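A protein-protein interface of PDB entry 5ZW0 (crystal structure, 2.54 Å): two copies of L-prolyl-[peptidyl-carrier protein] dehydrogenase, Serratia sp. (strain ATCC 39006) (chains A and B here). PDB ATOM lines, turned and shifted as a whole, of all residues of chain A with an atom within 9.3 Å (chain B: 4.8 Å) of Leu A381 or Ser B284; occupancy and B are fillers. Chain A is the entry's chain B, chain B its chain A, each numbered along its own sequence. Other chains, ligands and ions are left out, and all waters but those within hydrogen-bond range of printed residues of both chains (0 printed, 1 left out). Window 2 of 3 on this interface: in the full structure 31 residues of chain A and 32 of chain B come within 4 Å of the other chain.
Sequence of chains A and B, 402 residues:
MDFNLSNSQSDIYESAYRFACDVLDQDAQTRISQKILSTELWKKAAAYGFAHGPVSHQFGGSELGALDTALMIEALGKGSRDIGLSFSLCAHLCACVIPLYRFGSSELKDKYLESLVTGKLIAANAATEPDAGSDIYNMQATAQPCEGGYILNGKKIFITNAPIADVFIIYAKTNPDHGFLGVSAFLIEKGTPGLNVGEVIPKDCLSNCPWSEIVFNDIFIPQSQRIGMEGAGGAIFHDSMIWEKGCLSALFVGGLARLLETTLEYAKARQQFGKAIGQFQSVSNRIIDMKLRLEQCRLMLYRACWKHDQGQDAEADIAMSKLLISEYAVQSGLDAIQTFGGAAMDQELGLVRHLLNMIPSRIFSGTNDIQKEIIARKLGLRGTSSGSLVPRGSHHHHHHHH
O of Leu A381 sits close to OE1 of Gln B279.
O of Ala B267 is in hydrogen-bond range of N of Gly B278 (3.2 Å). The side-chain hydroxyl (OG) of Ser B284 lies close to the backbone carbonyl oxygen (O) of Gln B281, 3.4 Å away. O of Gln B281 lies close to ND2 of Asn B285 (3.2 Å). The side-chain carboxylate (OE1) of Glu A373 is in salt-bridge range of the guanidinium group (NE) of Arg A382. The backbone NH of Leu A381 sits at hydrogen-bond distance from the backbone carbonyl oxygen of Ala A376 (3.0 Å).
Asn B285 touches Lys A372. Lys A372 touches Ile B288 (O to CD1, 3.3 Å). Leu B264 touches Leu A379 (CD2 to O, 3.7 Å). Leu A379 touches Lys B268. CG2 of Ile B287 touches CD1 of Leu A379, at 3.98 Å. Lys B268 touches Gly A380. Leu A381 touches Leu B264 (CD2 to CD2, 3.8 Å). O of Gly B278 touches O of Leu A381 (3.9 Å). Leu A381 touches Ser B284. Arg A382 touches Gln B279 (CB to OE1, 3.1 Å).
Of the printed residues of chain B, Lys A372 touches Asn B285 and Ile B288. Lys A378 touches none of the printed residues of chain B. Of the printed residues of chain B, Gly A380 touches Lys B268 (3.7 Å). Ala B267 touches none of the printed residues of chain A. Of the printed residues of chain A, Gln B279 touches Leu A381 and Arg A382. No residue of chain A comes within 4 Å of Val B283. Ser B284 touches just one residue of chain A: Leu A381. Of the printed residues of chain A, Asn B285 touches Lys A372 (3.8 Å). Ile B287 touches just one residue of chain A: Leu A379. Printed residues of chain A within 4 Å of Ile B288: Lys A372 (3.3 Å). The nearest residue of chain B that does not touch Leu A381 is Ile B287 (4.1 Å).
Of the 13 printed residues of chain A, 5 touch a printed residue of chain B. Hydrophobic or aromatic side chains of chain A that line the printed part of chain B: Leu A379 and Leu A381. Of the 14 printed residues of chain B, 8 touch a printed residue of chain A. Among the printed residues, no Asp or Glu carboxylate lies within 4 Å of a Lys or Arg side-chain nitrogen of the other chain.
No position is printed for both chains. Of the 11 pairs that touch across the chains among the printed residues, none has its exchanged pair printed and touching as well.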
ATOM      1  N   LEU A 323      39.346 -32.302 -28.952  1.00  0.00           N
ATOM      2  CA  LEU A 323      38.911 -32.085 -27.580  1.00  0.00           C
ATOM      3  C   LEU A 323      38.794 -33.403 -26.831  1.00  0.00           C
ATOM      4  O   LEU A 323      39.394 -33.599 -25.759  1.00  0.00           O
ATOM      5  CB  LEU A 323      37.557 -31.377 -27.609  1.00  0.00           C
ATOM      6  CG  LEU A 323      36.967 -30.700 -26.395  1.00  0.00           C
ATOM      7  CD1 LEU A 323      38.050 -29.858 -25.807  1.00  0.00           C
ATOM      8  CD2 LEU A 323      35.806 -29.815 -26.860  1.00  0.00           C
ATOM      9  N   ASP A 369      40.158 -24.623 -25.229  1.00  0.00           N
ATOM     10  CA  ASP A 369      39.262 -23.473 -25.349  1.00  0.00           C
ATOM     11  C   ASP A 369      39.066 -23.054 -26.797  1.00  0.00           C
ATOM     12  O   ASP A 369      37.971 -22.611 -27.180  1.00  0.00           O
ATOM     13  CB  ASP A 369      39.793 -22.312 -24.519  1.00  0.00           C
ATOM     14  CG  ASP A 369      39.533 -22.498 -23.038  1.00  0.00           C
ATOM     15  OD1 ASP A 369      38.511 -23.128 -22.681  1.00  0.00           O
ATOM     16  OD2 ASP A 369      40.374 -22.055 -22.227  1.00  0.00           O
ATOM     17  N   LYS A 372      36.502 -25.421 -28.199  1.00  0.00           N
ATOM     18  CA  LYS A 372      35.179 -25.028 -27.719  1.00  0.00           C
ATOM     19  C   LYS A 372      34.646 -23.837 -28.506  1.00  0.00           C
ATOM     20  O   LYS A 372      33.456 -23.794 -28.847  1.00  0.00           O
ATOM     21  CB  LYS A 372      35.239 -24.729 -26.225  1.00  0.00           C
ATOM     22  CG  LYS A 372      35.246 -25.991 -25.368  1.00  0.00           C
ATOM     23  CD  LYS A 372      35.707 -25.700 -23.979  1.00  0.00           C
ATOM     24  CE  LYS A 372      35.657 -26.934 -23.093  1.00  0.00           C
ATOM     25  NZ  LYS A 372      34.249 -27.321 -22.771  1.00  0.00           N
ATOM     26  N   GLU A 373      35.523 -22.886 -28.852  1.00  0.00           N
ATOM     27  CA  GLU A 373      35.077 -21.744 -29.648  1.00  0.00           C
ATOM     28  C   GLU A 373      34.629 -22.172 -31.041  1.00  0.00           C
ATOM     29  O   GLU A 373      33.590 -21.710 -31.530  1.00  0.00           O
ATOM     30  CB  GLU A 373      36.196 -20.714 -29.745  1.00  0.00           C
ATOM     31  CG  GLU A 373      35.785 -19.237 -29.555  1.00  0.00           C
ATOM     32  CD  GLU A 373      35.077 -18.942 -28.222  1.00  0.00           C
ATOM     33  OE1 GLU A 373      33.952 -19.450 -28.026  1.00  0.00           O
ATOM     34  OE2 GLU A 373      35.658 -18.228 -27.363  1.00  0.00           O
ATOM     35  N   ILE A 374      35.381 -23.067 -31.687  1.00  0.00           N
ATOM     36  CA  ILE A 374      34.968 -23.561 -33.002  1.00  0.00           C
ATOM     37  C   ILE A 374      33.595 -24.217 -32.926  1.00  0.00           C
ATOM     38  O   ILE A 374      32.719 -23.975 -33.772  1.00  0.00           O
ATOM     39  CB  ILE A 374      36.010 -24.531 -33.570  1.00  0.00           C
ATOM     40  CG1 ILE A 374      37.298 -23.784 -33.881  1.00  0.00           C
ATOM     41  CG2 ILE A 374      35.433 -25.248 -34.797  1.00  0.00           C
ATOM     42  CD1 ILE A 374      38.530 -24.644 -33.785  1.00  0.00           C
ATOM     43  N   ILE A 375      33.394 -25.073 -31.913  1.00  0.00           N
ATOM     44  CA  ILE A 375      32.119 -25.782 -31.767  1.00  0.00           C
ATOM     45  C   ILE A 375      30.988 -24.801 -31.475  1.00  0.00           C
ATOM     46  O   ILE A 375      29.898 -24.888 -32.060  1.00  0.00           O
ATOM     47  CB  ILE A 375      32.232 -26.873 -30.681  1.00  0.00           C
ATOM     48  CG1 ILE A 375      33.207 -27.980 -31.120  1.00  0.00           C
ATOM     49  CG2 ILE A 375      30.861 -27.444 -30.336  1.00  0.00           C
ATOM     50  CD1 ILE A 375      33.862 -28.721 -29.993  1.00  0.00           C
ATOM     51  N   ALA A 376      31.225 -23.848 -30.571  1.00  0.00           N
ATOM     52  CA  ALA A 376      30.182 -22.881 -30.245  1.00  0.00           C
ATOM     53  C   ALA A 376      29.798 -22.064 -31.471  1.00  0.00           C
ATOM     54  O   ALA A 376      28.605 -21.850 -31.733  1.00  0.00           O
ATOM     55  CB  ALA A 376      30.633 -21.973 -29.106  1.00  0.00           C
ATOM     56  N   ARG A 377      30.792 -21.620 -32.252  1.00  0.00           N
ATOM     57  CA  ARG A 377      30.476 -20.892 -33.469  1.00  0.00           C
ATOM     58  C   ARG A 377      29.659 -21.755 -34.417  1.00  0.00           C
ATOM     59  O   ARG A 377      28.665 -21.295 -34.988  1.00  0.00           O
ATOM     60  CB  ARG A 377      31.744 -20.380 -34.129  1.00  0.00           C
ATOM     61  CG  ARG A 377      31.581 -20.158 -35.625  1.00  0.00           C
ATOM     62  CD  ARG A 377      32.632 -19.210 -36.182  1.00  0.00           C
ATOM     63  NE  ARG A 377      33.886 -19.239 -35.431  1.00  0.00           N
ATOM     64  CZ  ARG A 377      34.859 -20.124 -35.628  1.00  0.00           C
ATOM     65  NH1 ARG A 377      34.716 -21.067 -36.555  1.00  0.00           N
ATOM     66  NH2 ARG A 377      35.973 -20.068 -34.892  1.00  0.00           N
ATOM     67  N   LYS A 378      30.047 -23.020 -34.587  1.00  0.00           N
ATOM     68  CA  LYS A 378      29.262 -23.922 -35.427  1.00  0.00           C
ATOM     69  C   LYS A 378      27.838 -24.115 -34.910  1.00  0.00           C
ATOM     70  O   LYS A 378      26.926 -24.410 -35.698  1.00  0.00           O
ATOM     71  CB  LYS A 378      29.962 -25.274 -35.514  1.00  0.00           C
ATOM     72  CG  LYS A 378      29.285 -26.295 -36.435  1.00  0.00           C
ATOM     73  CD  LYS A 378      29.618 -26.052 -37.883  1.00  0.00           C
ATOM     74  CE  LYS A 378      29.282 -27.285 -38.697  1.00  0.00           C
ATOM     75  NZ  LYS A 378      29.915 -27.227 -40.039  1.00  0.00           N
ATOM     76  N   LEU A 379      27.624 -23.985 -33.601  1.00  0.00           N
ATOM     77  CA  LEU A 379      26.292 -24.176 -33.028  1.00  0.00           C
ATOM     78  C   LEU A 379      25.407 -22.929 -33.116  1.00  0.00           C
ATOM     79  O   LEU A 379      24.199 -23.021 -32.859  1.00  0.00           O
ATOM     80  CB  LEU A 379      26.424 -24.623 -31.565  1.00  0.00           C
ATOM     81  CG  LEU A 379      26.764 -26.101 -31.287  1.00  0.00           C
ATOM     82  CD1 LEU A 379      27.101 -26.354 -29.811  1.00  0.00           C
ATOM     83  CD2 LEU A 379      25.664 -27.047 -31.733  1.00  0.00           C
ATOM     84  N   GLY A 380      25.971 -21.781 -33.476  1.00  0.00           N
ATOM     85  CA  GLY A 380      25.218 -20.549 -33.534  1.00  0.00           C
ATOM     86  C   GLY A 380      25.249 -19.744 -32.257  1.00  0.00           C
ATOM     87  O   GLY A 380      24.327 -18.961 -32.010  1.00  0.00           O
ATOM     88  N   LEU A 381      26.301 -19.874 -31.453  1.00  0.00           N
ATOM     89  CA  LEU A 381      26.345 -19.264 -30.132  1.00  0.00           C
ATOM     90  C   LEU A 381      27.184 -17.998 -30.086  1.00  0.00           C
ATOM     91  O   LEU A 381      27.542 -17.551 -28.987  1.00  0.00           O
ATOM     92  CB  LEU A 381      26.874 -20.250 -29.093  1.00  0.00           C
ATOM     93  CG  LEU A 381      26.063 -21.451 -28.652  1.00  0.00           C
ATOM     94  CD1 LEU A 381      26.859 -22.224 -27.634  1.00  0.00           C
ATOM     95  CD2 LEU A 381      24.745 -21.013 -28.070  1.00  0.00           C
ATOM     96  N   ARG A 382      27.487 -17.405 -31.238  1.00  0.00           N
ATOM     97  CA  ARG A 382      28.233 -16.148 -31.278  1.00  0.00           C
ATOM     98  C   ARG A 382      28.442 -15.656 -32.709  1.00  0.00           C
ATOM     99  O   ARG A 382      28.485 -14.450 -32.955  1.00  0.00           O
ATOM    100  CB  ARG A 382      29.584 -16.301 -30.563  1.00  0.00           C
ATOM    101  CG  ARG A 382      30.531 -17.300 -31.186  1.00  0.00           C
ATOM    102  CD  ARG A 382      31.738 -17.535 -30.281  1.00  0.00           C
ATOM    103  NE  ARG A 382      31.379 -18.256 -29.061  1.00  0.00           N
ATOM    104  CZ  ARG A 382      31.384 -17.729 -27.841  1.00  0.00           C
ATOM    105  NH1 ARG A 382      31.050 -18.473 -26.789  1.00  0.00           N
ATOM    106  NH2 ARG A 382      31.735 -16.462 -27.675  1.00  0.00           N
ATOM    107  N   LEU B 264      19.654 -24.939 -26.870  1.00  0.00           N
ATOM    108  CA  LEU B 264      20.256 -24.016 -27.819  1.00  0.00           C
ATOM    109  C   LEU B 264      19.348 -22.814 -28.050  1.00  0.00           C
ATOM    110  O   LEU B 264      19.799 -21.664 -27.996  1.00  0.00           O
ATOM    111  CB  LEU B 264      20.554 -24.727 -29.128  1.00  0.00           C
ATOM    112  CG  LEU B 264      21.964 -25.140 -29.505  1.00  0.00           C
ATOM    113  CD1 LEU B 264      21.885 -25.723 -30.893  1.00  0.00           C
ATOM    114  CD2 LEU B 264      22.888 -23.952 -29.496  1.00  0.00           C
ATOM    115  N   ALA B 267      19.226 -20.426 -25.346  1.00  0.00           N
ATOM    116  CA  ALA B 267      20.492 -19.725 -25.185  1.00  0.00           C
ATOM    117  C   ALA B 267      20.707 -18.662 -26.250  1.00  0.00           C
ATOM    118  O   ALA B 267      21.358 -17.646 -25.979  1.00  0.00           O
ATOM    119  CB  ALA B 267      21.663 -20.710 -25.195  1.00  0.00           C
ATOM    120  N   LYS B 268      20.195 -18.875 -27.460  1.00  0.00           N
ATOM    121  CA  LYS B 268      20.390 -17.862 -28.483  1.00  0.00           C
ATOM    122  C   LYS B 268      19.507 -16.644 -28.244  1.00  0.00           C
ATOM    123  O   LYS B 268      19.828 -15.551 -28.724  1.00  0.00           O
ATOM    124  CB  LYS B 268      20.103 -18.439 -29.863  1.00  0.00           C
ATOM    125  CG  LYS B 268      21.069 -19.479 -30.383  1.00  0.00           C
ATOM    126  CD  LYS B 268      20.414 -20.151 -31.577  1.00  0.00           C
ATOM    127  CE  LYS B 268      21.224 -21.305 -32.150  1.00  0.00           C
ATOM    128  NZ  LYS B 268      20.420 -22.053 -33.168  1.00  0.00           N
ATOM    129  N   GLY B 278      24.003 -17.343 -24.171  1.00  0.00           N
ATOM    130  CA  GLY B 278      24.862 -18.368 -24.739  1.00  0.00           C
ATOM    131  C   GLY B 278      26.276 -17.909 -25.018  1.00  0.00           C
ATOM    132  O   GLY B 278      27.150 -18.753 -25.249  1.00  0.00           O
ATOM    133  N   GLN B 279      26.519 -16.600 -25.002  1.00  0.00           N
ATOM    134  CA  GLN B 279      27.872 -16.071 -25.067  1.00  0.00           C
ATOM    135  C   GLN B 279      28.576 -16.111 -23.714  1.00  0.00           C
ATOM    136  O   GLN B 279      29.788 -15.870 -23.658  1.00  0.00           O
ATOM    137  CB  GLN B 279      27.838 -14.636 -25.608  1.00  0.00           C
ATOM    138  CG  GLN B 279      26.874 -14.431 -26.785  1.00  0.00           C
ATOM    139  CD  GLN B 279      27.585 -14.065 -28.076  1.00  0.00           C
ATOM    140  OE1 GLN B 279      28.742 -14.423 -28.282  1.00  0.00           O
ATOM    141  NE2 GLN B 279      26.887 -13.354 -28.957  1.00  0.00           N
ATOM    142  N   PHE B 280      27.854 -16.427 -22.634  1.00  0.00           N
ATOM    143  CA  PHE B 280      28.453 -16.618 -21.315  1.00  0.00           C
ATOM    144  C   PHE B 280      29.008 -18.034 -21.230  1.00  0.00           C
ATOM    145  O   PHE B 280      28.253 -19.003 -21.369  1.00  0.00           O
ATOM    146  CB  PHE B 280      27.417 -16.381 -20.215  1.00  0.00           C
ATOM    147  CG  PHE B 280      27.156 -14.927 -19.929  1.00  0.00           C
ATOM    148  CD1 PHE B 280      27.916 -14.236 -18.997  1.00  0.00           C
ATOM    149  CD2 PHE B 280      26.148 -14.251 -20.599  1.00  0.00           C
ATOM    150  CE1 PHE B 280      27.670 -12.900 -18.742  1.00  0.00           C
ATOM    151  CE2 PHE B 280      25.901 -12.916 -20.348  1.00  0.00           C
ATOM    152  CZ  PHE B 280      26.664 -12.242 -19.423  1.00  0.00           C
ATOM    153  N   GLN B 281      30.321 -18.154 -20.981  1.00  0.00           N
ATOM    154  CA  GLN B 281      31.008 -19.429 -21.190  1.00  0.00           C
ATOM    155  C   GLN B 281      30.488 -20.552 -20.299  1.00  0.00           C
ATOM    156  O   GLN B 281      30.760 -21.723 -20.589  1.00  0.00           O
ATOM    157  CB  GLN B 281      32.519 -19.293 -20.979  1.00  0.00           C
ATOM    158  CG  GLN B 281      33.292 -18.724 -22.156  1.00  0.00           C
ATOM    159  CD  GLN B 281      34.790 -18.800 -21.934  1.00  0.00           C
ATOM    160  OE1 GLN B 281      35.252 -19.430 -20.976  1.00  0.00           O
ATOM    161  NE2 GLN B 281      35.558 -18.152 -22.807  1.00  0.00           N
ATOM    162  N   SER B 282      29.734 -20.237 -19.241  1.00  0.00           N
ATOM    163  CA  SER B 282      29.113 -21.280 -18.430  1.00  0.00           C
ATOM    164  C   SER B 282      28.024 -22.009 -19.214  1.00  0.00           C
ATOM    165  O   SER B 282      28.050 -23.242 -19.353  1.00  0.00           O
ATOM    166  CB  SER B 282      28.540 -20.664 -17.158  1.00  0.00           C
ATOM    167  OG  SER B 282      27.706 -19.558 -17.481  1.00  0.00           O
ATOM    168  N   VAL B 283      27.062 -21.254 -19.750  1.00  0.00           N
ATOM    169  CA  VAL B 283      25.970 -21.864 -20.495  1.00  0.00           C
ATOM    170  C   VAL B 283      26.494 -22.527 -21.767  1.00  0.00           C
ATOM    171  O   VAL B 283      26.080 -23.641 -22.123  1.00  0.00           O
ATOM    172  CB  VAL B 283      24.891 -20.805 -20.804  1.00  0.00           C
ATOM    173  CG1 VAL B 283      23.782 -21.378 -21.690  1.00  0.00           C
ATOM    174  CG2 VAL B 283      24.310 -20.248 -19.516  1.00  0.00           C
ATOM    175  N   SER B 284      27.423 -21.865 -22.461  1.00  0.00           N
ATOM    176  CA  SER B 284      27.958 -22.432 -23.692  1.00  0.00           C
ATOM    177  C   SER B 284      28.784 -23.681 -23.409  1.00  0.00           C
ATOM    178  O   SER B 284      28.770 -24.629 -24.198  1.00  0.00           O
ATOM    179  CB  SER B 284      28.774 -21.391 -24.455  1.00  0.00           C
ATOM    180  OG  SER B 284      30.058 -21.236 -23.885  1.00  0.00           O
ATOM    181  N   ASN B 285      29.522 -23.709 -22.302  1.00  0.00           N
ATOM    182  CA  ASN B 285      30.254 -24.927 -21.996  1.00  0.00           C
ATOM    183  C   ASN B 285      29.293 -26.071 -21.698  1.00  0.00           C
ATOM    184  O   ASN B 285      29.552 -27.227 -22.081  1.00  0.00           O
ATOM    185  CB  ASN B 285      31.214 -24.703 -20.827  1.00  0.00           C
ATOM    186  CG  ASN B 285      32.492 -23.998 -21.245  1.00  0.00           C
ATOM    187  OD1 ASN B 285      32.775 -23.826 -22.442  1.00  0.00           O
ATOM    188  ND2 ASN B 285      33.290 -23.610 -20.260  1.00  0.00           N
ATOM    189  N   ARG B 286      28.168 -25.764 -21.039  1.00  0.00           N
ATOM    190  CA  ARG B 286      27.169 -26.795 -20.788  1.00  0.00           C
ATOM    191  C   ARG B 286      26.560 -27.305 -22.093  1.00  0.00           C
ATOM    192  O   ARG B 286      26.351 -28.518 -22.265  1.00  0.00           O
ATOM    193  CB  ARG B 286      26.110 -26.258 -19.829  1.00  0.00           C
ATOM    194  CG  ARG B 286      26.565 -26.358 -18.344  1.00  0.00           C
ATOM    195  CD  ARG B 286      25.426 -26.126 -17.337  1.00  0.00           C
ATOM    196  NE  ARG B 286      25.243 -24.716 -17.032  1.00  0.00           N
ATOM    197  CZ  ARG B 286      25.937 -24.081 -16.095  1.00  0.00           C
ATOM    198  NH1 ARG B 286      26.842 -24.740 -15.378  1.00  0.00           N
ATOM    199  NH2 ARG B 286      25.734 -22.792 -15.883  1.00  0.00           N
ATOM    200  N   ILE B 287      26.339 -26.406 -23.054  1.00  0.00           N
ATOM    201  CA  ILE B 287      25.797 -26.823 -24.348  1.00  0.00           C
ATOM    202  C   ILE B 287      26.812 -27.662 -25.137  1.00  0.00           C
ATOM    203  O   ILE B 287      26.457 -28.655 -25.783  1.00  0.00           O
ATOM    204  CB  ILE B 287      25.354 -25.593 -25.149  1.00  0.00           C
ATOM    205  CG1 ILE B 287      24.236 -24.856 -24.400  1.00  0.00           C
ATOM    206  CG2 ILE B 287      24.881 -26.027 -26.527  1.00  0.00           C
ATOM    207  CD1 ILE B 287      23.610 -23.747 -25.193  1.00  0.00           C
ATOM    208  N   ILE B 288      28.074 -27.249 -25.131  1.00  0.00           N
ATOM    209  CA  ILE B 288      29.119 -27.994 -25.810  1.00  0.00           C
ATOM    210  C   ILE B 288      29.246 -29.401 -25.218  1.00  0.00           C
ATOM    211  O   ILE B 288      29.367 -30.392 -25.950  1.00  0.00           O
ATOM    212  CB  ILE B 288      30.428 -27.183 -25.754  1.00  0.00           C
ATOM    213  CG1 ILE B 288      30.290 -25.964 -26.637  1.00  0.00           C
ATOM    214  CG2 ILE B 288      31.637 -27.996 -26.171  1.00  0.00           C
ATOM    215  CD1 ILE B 288      31.442 -25.002 -26.468  1.00  0.00           C
